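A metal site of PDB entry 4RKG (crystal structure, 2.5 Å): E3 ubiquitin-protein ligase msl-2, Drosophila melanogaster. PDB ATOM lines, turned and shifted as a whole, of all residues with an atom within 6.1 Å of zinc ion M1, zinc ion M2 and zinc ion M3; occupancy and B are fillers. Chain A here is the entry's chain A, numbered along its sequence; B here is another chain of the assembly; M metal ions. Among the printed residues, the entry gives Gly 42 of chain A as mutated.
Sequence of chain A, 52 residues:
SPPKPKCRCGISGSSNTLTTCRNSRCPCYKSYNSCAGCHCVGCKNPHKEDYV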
ATOM      1  N   LYS A   6      20.655 -16.293 -10.836  1.00  0.00           N
ATOM      2  CA  LYS A   6      19.927 -17.555 -10.554  1.00  0.00           C
ATOM      3  C   LYS A   6      20.591 -18.796 -11.193  1.00  0.00           C
ATOM      4  O   LYS A   6      20.338 -19.088 -12.361  1.00  0.00           O
ATOM      5  CB  LYS A   6      18.478 -17.455 -11.064  1.00  0.00           C
ATOM      6  CG  LYS A   6      17.426 -17.112 -10.005  1.00  0.00           C
ATOM      7  CD  LYS A   6      16.077 -16.780 -10.646  1.00  0.00           C
ATOM      8  CE  LYS A   6      15.949 -15.281 -10.936  1.00  0.00           C
ATOM      9  NZ  LYS A   6      16.028 -14.455  -9.692  1.00  0.00           N
ATOM     10  N   CYS A   7      21.404 -19.533 -10.422  1.00  0.00           N
ATOM     11  CA  CYS A   7      22.239 -20.621 -10.971  1.00  0.00           C
ATOM     12  C   CYS A   7      21.489 -21.940 -11.197  1.00  0.00           C
ATOM     13  O   CYS A   7      20.276 -22.050 -10.944  1.00  0.00           O
ATOM     14  CB  CYS A   7      23.483 -20.880 -10.095  1.00  0.00           C
ATOM     15  SG  CYS A   7      23.295 -21.454  -8.382  1.00  0.00           S
ATOM     16  N   ARG A   8      22.214 -22.922 -11.716  1.00  0.00           N
ATOM     17  CA  ARG A   8      21.664 -24.231 -11.991  1.00  0.00           C
ATOM     18  C   ARG A   8      22.739 -25.316 -11.798  1.00  0.00           C
ATOM     19  O   ARG A   8      22.805 -26.290 -12.565  1.00  0.00           O
ATOM     20  CB  ARG A   8      21.066 -24.265 -13.412  1.00  0.00           C
ATOM     21  CG  ARG A   8      19.585 -23.909 -13.436  1.00  0.00           C
ATOM     22  CD  ARG A   8      19.057 -23.757 -14.872  1.00  0.00           C
ATOM     23  NE  ARG A   8      19.188 -24.982 -15.647  1.00  0.00           N
ATOM     24  CZ  ARG A   8      19.718 -25.054 -16.866  1.00  0.00           C
ATOM     25  NH1 ARG A   8      19.811 -26.230 -17.486  1.00  0.00           N
ATOM     26  NH2 ARG A   8      20.165 -23.955 -17.455  1.00  0.00           N
ATOM     27  N   CYS A   9      23.566 -25.132 -10.774  1.00  0.00           N
ATOM     28  CA  CYS A   9      24.585 -26.104 -10.363  1.00  0.00           C
ATOM     29  C   CYS A   9      23.955 -27.340  -9.723  1.00  0.00           C
ATOM     30  O   CYS A   9      23.103 -27.214  -8.869  1.00  0.00           O
ATOM     31  CB  CYS A   9      25.572 -25.482  -9.366  1.00  0.00           C
ATOM     32  SG  CYS A   9      26.097 -23.778  -9.711  1.00  0.00           S
ATOM     33  N   THR A  20      29.528 -27.861  -4.733  1.00  0.00           N
ATOM     34  CA  THR A  20      28.404 -27.324  -5.497  1.00  0.00           C
ATOM     35  C   THR A  20      27.954 -25.977  -4.958  1.00  0.00           C
ATOM     36  O   THR A  20      27.585 -25.842  -3.785  1.00  0.00           O
ATOM     37  CB  THR A  20      27.182 -28.260  -5.484  1.00  0.00           C
ATOM     38  OG1 THR A  20      27.441 -29.398  -6.312  1.00  0.00           O
ATOM     39  CG2 THR A  20      25.969 -27.533  -6.021  1.00  0.00           C
ATOM     40  N   CYS A  21      28.013 -24.963  -5.822  1.00  0.00           N
ATOM     41  CA  CYS A  21      27.775 -23.570  -5.456  1.00  0.00           C
ATOM     42  C   CYS A  21      28.765 -23.125  -4.383  1.00  0.00           C
ATOM     43  O   CYS A  21      28.512 -22.175  -3.643  1.00  0.00           O
ATOM     44  CB  CYS A  21      26.341 -23.354  -4.962  1.00  0.00           C
ATOM     45  SG  CYS A  21      25.046 -23.756  -6.152  1.00  0.00           S
ATOM     46  N   ARG A  22      29.894 -23.815  -4.294  1.00  0.00           N
ATOM     47  CA  ARG A  22      30.950 -23.395  -3.380  1.00  0.00           C
ATOM     48  C   ARG A  22      32.235 -23.163  -4.174  1.00  0.00           C
ATOM     49  O   ARG A  22      33.310 -23.482  -3.700  1.00  0.00           O
ATOM     50  CB  ARG A  22      31.175 -24.425  -2.275  1.00  0.00           C
ATOM     51  CG  ARG A  22      31.872 -23.859  -1.052  1.00  0.00           C
ATOM     52  CD  ARG A  22      32.405 -24.928  -0.146  1.00  0.00           C
ATOM     53  NE  ARG A  22      32.797 -24.355   1.137  1.00  0.00           N
ATOM     54  CZ  ARG A  22      31.967 -24.178   2.147  1.00  0.00           C
ATOM     55  NH1 ARG A  22      30.696 -24.539   2.043  1.00  0.00           N
ATOM     56  NH2 ARG A  22      32.407 -23.646   3.283  1.00  0.00           N
ATOM     57  N   CYS A  26      30.288 -21.271 -10.076  1.00  0.00           N
ATOM     58  CA  CYS A  26      28.952 -20.815  -9.706  1.00  0.00           C
ATOM     59  C   CYS A  26      28.939 -19.292  -9.613  1.00  0.00           C
ATOM     60  O   CYS A  26      29.786 -18.725  -8.935  1.00  0.00           O
ATOM     61  CB  CYS A  26      28.500 -21.451  -8.373  1.00  0.00           C
ATOM     62  SG  CYS A  26      27.025 -20.716  -7.579  1.00  0.00           S
ATOM     63  N   PRO A  27      28.005 -18.646 -10.308  1.00  0.00           N
ATOM     64  CA  PRO A  27      27.846 -17.185 -10.346  1.00  0.00           C
ATOM     65  C   PRO A  27      27.649 -16.535  -8.998  1.00  0.00           C
ATOM     66  O   PRO A  27      28.425 -15.660  -8.614  1.00  0.00           O
ATOM     67  CB  PRO A  27      26.586 -16.983 -11.204  1.00  0.00           C
ATOM     68  CG  PRO A  27      26.014 -18.338 -11.428  1.00  0.00           C
ATOM     69  CD  PRO A  27      27.142 -19.296 -11.297  1.00  0.00           C
ATOM     70  N   CYS A  28      26.606 -16.959  -8.297  1.00  0.00           N
ATOM     71  CA  CYS A  28      26.255 -16.404  -6.992  1.00  0.00           C
ATOM     72  C   CYS A  28      27.425 -16.457  -6.005  1.00  0.00           C
ATOM     73  O   CYS A  28      27.716 -15.467  -5.328  1.00  0.00           O
ATOM     74  CB  CYS A  28      25.054 -17.171  -6.432  1.00  0.00           C
ATOM     75  SG  CYS A  28      24.077 -18.020  -7.713  1.00  0.00           S
ATOM     76  N   TYR A  29      28.089 -17.606  -5.941  1.00  0.00           N
ATOM     77  CA  TYR A  29      29.300 -17.750  -5.154  1.00  0.00           C
ATOM     78  C   TYR A  29      30.306 -16.679  -5.567  1.00  0.00           C
ATOM     79  O   TYR A  29      30.713 -15.854  -4.761  1.00  0.00           O
ATOM     80  CB  TYR A  29      29.919 -19.141  -5.339  1.00  0.00           C
ATOM     81  CG  TYR A  29      30.849 -19.581  -4.234  1.00  0.00           C
ATOM     82  CD1 TYR A  29      30.358 -19.923  -2.974  1.00  0.00           C
ATOM     83  CD2 TYR A  29      32.214 -19.669  -4.436  1.00  0.00           C
ATOM     84  CE1 TYR A  29      31.196 -20.341  -1.958  1.00  0.00           C
ATOM     85  CE2 TYR A  29      33.072 -20.085  -3.418  1.00  0.00           C
ATOM     86  CZ  TYR A  29      32.554 -20.426  -2.183  1.00  0.00           C
ATOM     87  OH  TYR A  29      33.392 -20.844  -1.167  1.00  0.00           O
ATOM     88  N   ASN A  33      27.108 -13.739  -3.680  1.00  0.00           N
ATOM     89  CA  ASN A  33      25.706 -13.739  -3.280  1.00  0.00           C
ATOM     90  C   ASN A  33      25.217 -15.142  -2.975  1.00  0.00           C
ATOM     91  O   ASN A  33      25.869 -16.122  -3.341  1.00  0.00           O
ATOM     92  CB  ASN A  33      24.831 -13.112  -4.374  1.00  0.00           C
ATOM     93  CG  ASN A  33      25.331 -11.763  -4.787  1.00  0.00           C
ATOM     94  OD1 ASN A  33      26.000 -11.630  -5.811  1.00  0.00           O
ATOM     95  ND2 ASN A  33      25.028 -10.740  -3.975  1.00  0.00           N
ATOM     96  N   SER A  34      24.083 -15.241  -2.286  1.00  0.00           N
ATOM     97  CA  SER A  34      23.498 -16.525  -1.915  1.00  0.00           C
ATOM     98  C   SER A  34      22.728 -17.143  -3.080  1.00  0.00           C
ATOM     99  O   SER A  34      22.662 -16.558  -4.164  1.00  0.00           O
ATOM    100  CB  SER A  34      22.560 -16.360  -0.712  1.00  0.00           C
ATOM    101  OG  SER A  34      21.427 -15.574  -1.070  1.00  0.00           O
ATOM    102  N   CYS A  35      22.150 -18.310  -2.870  1.00  0.00           N
ATOM    103  CA  CYS A  35      21.356 -18.946  -3.922  1.00  0.00           C
ATOM    104  C   CYS A  35      19.877 -18.782  -3.637  1.00  0.00           C
ATOM    105  O   CYS A  35      19.086 -19.710  -3.795  1.00  0.00           O
ATOM    106  CB  CYS A  35      21.726 -20.412  -4.073  1.00  0.00           C
ATOM    107  SG  CYS A  35      23.294 -20.640  -4.854  1.00  0.00           S
ATOM    108  N   ALA A  36      19.502 -17.588  -3.193  1.00  0.00           N
ATOM    109  CA  ALA A  36      18.106 -17.235  -3.023  1.00  0.00           C
ATOM    110  C   ALA A  36      17.397 -17.273  -4.375  1.00  0.00           C
ATOM    111  O   ALA A  36      17.713 -16.476  -5.263  1.00  0.00           O
ATOM    112  CB  ALA A  36      17.993 -15.851  -2.378  1.00  0.00           C
ATOM    113  N   CYS A  38      17.539 -19.613  -6.608  1.00  0.00           N
ATOM    114  CA  CYS A  38      18.265 -20.435  -7.576  1.00  0.00           C
ATOM    115  C   CYS A  38      17.598 -21.792  -7.843  1.00  0.00           C
ATOM    116  O   CYS A  38      16.665 -22.176  -7.158  1.00  0.00           O
ATOM    117  CB  CYS A  38      19.708 -20.670  -7.110  1.00  0.00           C
ATOM    118  SG  CYS A  38      20.898 -19.294  -7.310  1.00  0.00           S
ATOM    119  N   HIS A  39      18.100 -22.512  -8.827  1.00  0.00           N
ATOM    120  CA  HIS A  39      17.529 -23.812  -9.185  1.00  0.00           C
ATOM    121  C   HIS A  39      18.545 -24.945  -9.032  1.00  0.00           C
ATOM    122  O   HIS A  39      18.319 -26.064  -9.477  1.00  0.00           O
ATOM    123  CB  HIS A  39      16.977 -23.726 -10.611  1.00  0.00           C
ATOM    124  CG  HIS A  39      15.705 -22.971 -10.679  1.00  0.00           C
ATOM    125  ND1 HIS A  39      15.347 -22.190 -11.758  1.00  0.00           N
ATOM    126  CD2 HIS A  39      14.701 -22.835  -9.771  1.00  0.00           C
ATOM    127  CE1 HIS A  39      14.168 -21.631 -11.518  1.00  0.00           C
ATOM    128  NE2 HIS A  39      13.762 -22.006 -10.320  1.00  0.00           N
ATOM    129  N   CYS A  40      19.653 -24.617  -8.396  1.00  0.00           N
ATOM    130  CA  CYS A  40      20.678 -25.567  -7.980  1.00  0.00           C
ATOM    131  C   CYS A  40      20.139 -26.749  -7.165  1.00  0.00           C
ATOM    132  O   CYS A  40      19.030 -26.720  -6.630  1.00  0.00           O
ATOM    133  CB  CYS A  40      21.748 -24.822  -7.177  1.00  0.00           C
ATOM    134  SG  CYS A  40      21.069 -23.634  -5.952  1.00  0.00           S
ATOM    135  N   VAL A  41      20.938 -27.799  -7.069  1.00  0.00           N
ATOM    136  CA  VAL A  41      20.570 -29.017  -6.354  1.00  0.00           C
ATOM    137  C   VAL A  41      21.763 -29.406  -5.494  1.00  0.00           C
ATOM    138  O   VAL A  41      22.896 -29.381  -5.960  1.00  0.00           O
ATOM    139  CB  VAL A  41      20.210 -30.166  -7.328  1.00  0.00           C
ATOM    140  CG1 VAL A  41      19.834 -31.406  -6.605  1.00  0.00           C
ATOM    141  CG2 VAL A  41      19.077 -29.746  -8.275  1.00  0.00           C
ATOM    142  N   GLY A  42      21.515 -29.735  -4.240  1.00  0.00           N
ATOM    143  CA  GLY A  42      22.602 -30.066  -3.338  1.00  0.00           C
ATOM    144  C   GLY A  42      23.512 -28.854  -3.205  1.00  0.00           C
ATOM    145  O   GLY A  42      24.736 -28.981  -3.238  1.00  0.00           O
ATOM    146  N   CYS A  43      22.891 -27.692  -3.077  1.00  0.00           N
ATOM    147  CA  CYS A  43      23.612 -26.437  -2.877  1.00  0.00           C
ATOM    148  C   CYS A  43      24.434 -26.475  -1.608  1.00  0.00           C
ATOM    149  O   CYS A  43      23.961 -26.928  -0.578  1.00  0.00           O
ATOM    150  CB  CYS A  43      22.643 -25.260  -2.826  1.00  0.00           C
ATOM    151  SG  CYS A  43      23.529 -23.657  -2.752  1.00  0.00           S
ATOM    152  N   LYS A  44      25.665 -25.997  -1.681  1.00  0.00           N
ATOM    153  CA  LYS A  44      26.518 -25.935  -0.510  1.00  0.00           C
ATOM    154  C   LYS A  44      27.084 -24.533  -0.429  1.00  0.00           C
ATOM    155  O   LYS A  44      28.117 -24.296   0.183  1.00  0.00           O
ATOM    156  CB  LYS A  44      27.626 -26.984  -0.582  1.00  0.00           C
ATOM    157  CG  LYS A  44      27.149 -28.410  -0.833  1.00  0.00           C
ATOM    158  CD  LYS A  44      27.260 -29.259   0.401  1.00  0.00           C
ATOM    159  CE  LYS A  44      27.697 -30.699   0.107  1.00  0.00           C
ATOM    160  NZ  LYS A  44      26.908 -31.370  -0.948  1.00  0.00           N
ATOM    161  N   ASN A  45      26.398 -23.600  -1.064  1.00  0.00           N
ATOM    162  CA  ASN A  45      26.712 -22.193  -0.937  1.00  0.00           C
ATOM    163  C   ASN A  45      26.548 -21.737   0.501  1.00  0.00           C
ATOM    164  O   ASN A  45      25.435 -21.726   1.009  1.00  0.00           O
ATOM    165  CB  ASN A  45      25.815 -21.367  -1.846  1.00  0.00           C
ATOM    166  CG  ASN A  45      26.289 -19.947  -1.997  1.00  0.00           C
ATOM    167  OD1 ASN A  45      27.004 -19.423  -1.140  1.00  0.00           O
ATOM    168  ND2 ASN A  45      25.913 -19.307  -3.100  1.00  0.00           N
ATOM    169  P    DG B   5      28.006 -27.154 -12.008  1.00  0.00           P
ATOM    170  OP1  DG B   5      28.784 -26.906 -10.768  1.00  0.00           O
ATOM    171  OP2  DG B   5      26.909 -28.145 -12.034  1.00  0.00           O
ATOM    172  O5'  DG B   5      27.446 -25.755 -12.534  1.00  0.00           O
ATOM    173  C5'  DG B   5      28.340 -24.678 -12.663  1.00  0.00           C
ATOM    174  C4'  DG B   5      27.894 -23.705 -13.733  1.00  0.00           C
ATOM    175  O4'  DG B   5      28.136 -24.266 -15.047  1.00  0.00           O
ATOM    176  C3'  DG B   5      26.421 -23.352 -13.733  1.00  0.00           C
ATOM    177  O3'  DG B   5      26.316 -22.067 -14.270  1.00  0.00           O
ATOM    178  C2'  DG B   5      25.829 -24.409 -14.667  1.00  0.00           C
ATOM    179  C1'  DG B   5      26.917 -24.489 -15.718  1.00  0.00           C
ATOM    180  N9   DG B   5      27.024 -25.790 -16.323  1.00  0.00           N
ATOM    181  C8   DG B   5      26.983 -27.008 -15.686  1.00  0.00           C
ATOM    182  N7   DG B   5      27.171 -28.015 -16.489  1.00  0.00           N
ATOM    183  C5   DG B   5      27.390 -27.422 -17.724  1.00  0.00           C
ATOM    184  C6   DG B   5      27.649 -28.011 -18.982  1.00  0.00           C
ATOM    185  O6   DG B   5      27.746 -29.221 -19.246  1.00  0.00           O
ATOM    186  N1   DG B   5      27.796 -27.053 -19.979  1.00  0.00           N
ATOM    187  C2   DG B   5      27.689 -25.701 -19.782  1.00  0.00           C
ATOM    188  N2   DG B   5      27.855 -24.932 -20.878  1.00  0.00           N
ATOM    189  N3   DG B   5      27.448 -25.136 -18.619  1.00  0.00           N
ATOM    190  C4   DG B   5      27.308 -26.059 -17.632  1.00  0.00           C
ATOM    191  P    DC B   6      24.893 -21.377 -14.434  1.00  0.00           P
ATOM    192  OP1  DC B   6      25.154 -19.940 -14.182  1.00  0.00           O
ATOM    193  OP2  DC B   6      23.862 -22.107 -13.672  1.00  0.00           O
ATOM    194  O5'  DC B   6      24.588 -21.564 -15.981  1.00  0.00           O
ATOM    195  C5'  DC B   6      25.465 -21.011 -16.929  1.00  0.00           C
ATOM    196  C4'  DC B   6      24.955 -21.281 -18.319  1.00  0.00           C
ATOM    197  O4'  DC B   6      25.125 -22.695 -18.615  1.00  0.00           O
ATOM    198  C3'  DC B   6      23.469 -20.978 -18.540  1.00  0.00           C
ATOM    199  O3'  DC B   6      23.294 -20.542 -19.864  1.00  0.00           O
ATOM    200  C2'  DC B   6      22.840 -22.360 -18.338  1.00  0.00           C
ATOM    201  C1'  DC B   6      23.879 -23.201 -19.053  1.00  0.00           C
ATOM    202  N1   DC B   6      23.828 -24.656 -18.760  1.00  0.00           N
ATOM    203  C2   DC B   6      24.172 -25.555 -19.765  1.00  0.00           C
ATOM    204  O2   DC B   6      24.514 -25.110 -20.858  1.00  0.00           O
ATOM    205  N3   DC B   6      24.150 -26.875 -19.517  1.00  0.00           N
ATOM    206  C4   DC B   6      23.789 -27.307 -18.299  1.00  0.00           C
ATOM    207  N4   DC B   6      23.774 -28.632 -18.093  1.00  0.00           N
ATOM    208  C5   DC B   6      23.418 -26.407 -17.255  1.00  0.00           C
ATOM    209  C6   DC B   6      23.455 -25.094 -17.521  1.00  0.00           C
HETATM  210 ZN    ZN M   1      23.339 -23.051  -4.916  1.00  0.00          ZN
HETATM  211 ZN    ZN M   2      25.374 -22.321  -8.003  1.00  0.00          ZN
HETATM  212 ZN    ZN M   3      22.946 -19.975  -6.963  1.00  0.00          ZN
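Zinc ion M3 is bound by the side-chain sulfur of Cys 7 (2.1 Å), the side-chain sulfur of Cys 38 (2.2 Å), the side-chain sulfur of Cys 35 (2.2 Å) and the side-chain sulfur of Cys 28 (2.4 Å).
The backbone carbonyl oxygen of Cys 7 sits at hydrogen-bond distance from the backbone NH of His 39 (3.1 Å). ND2 of Asn 45 sits close to SG of Cys 35, 3.4 Å away. N of Asn 45 lies close to SG of Cys 43, 3.3 Å away. The side-chain sulfur (SG) of Cys 26 sits close to the backbone NH (N) of Tyr 29 (3.7 Å). The backbone NH (N) of Val 41 sits at hydrogen-bond distance from the backbone carbonyl oxygen (O) of Cys 9 (2.9 Å). O5' of DG 5 of chain B lies close to the side-chain sulfur of Cys 9 (3.7 Å). O of Cys 28 is in hydrogen-bond range of N of Asn 33 (2.5 Å).
Four residues have an atom within 4 Å of zinc ion M2: Cys 7, Cys 9, Cys 21 and Cys 26.
Zinc ion M1 is bound by the side-chain sulfur (SG) of Cys 21 (2.2 Å). Zinc ion M1 is bound by the side-chain sulfur (SG) of Cys 43 (2.3 Å). Zinc ion M1 is bound by the side-chain sulfur (SG) of Cys 35, 2.4 Å away. SG of Cys 40 is bound to zinc ion M1 (2.6 Å). Zinc ion M1 has four donor atoms within binding distance.
Within 4 Å of zinc ion M1: Cys 7, Cys 21, Cys 35, Cys 40 and Cys 43.
The side-chain sulfur (SG) of Cys 7 is bound to zinc ion M2. SG of Cys 26 is bound to zinc ion M2 (2.3 Å). SG of Cys 9 is bound to zinc ion M2 (2.4 Å). Zinc ion M2 is bound by the side-chain sulfur (SG) of Cys 21, at 2.4 Å. Zinc ion M2 has four donor atoms within binding distance.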
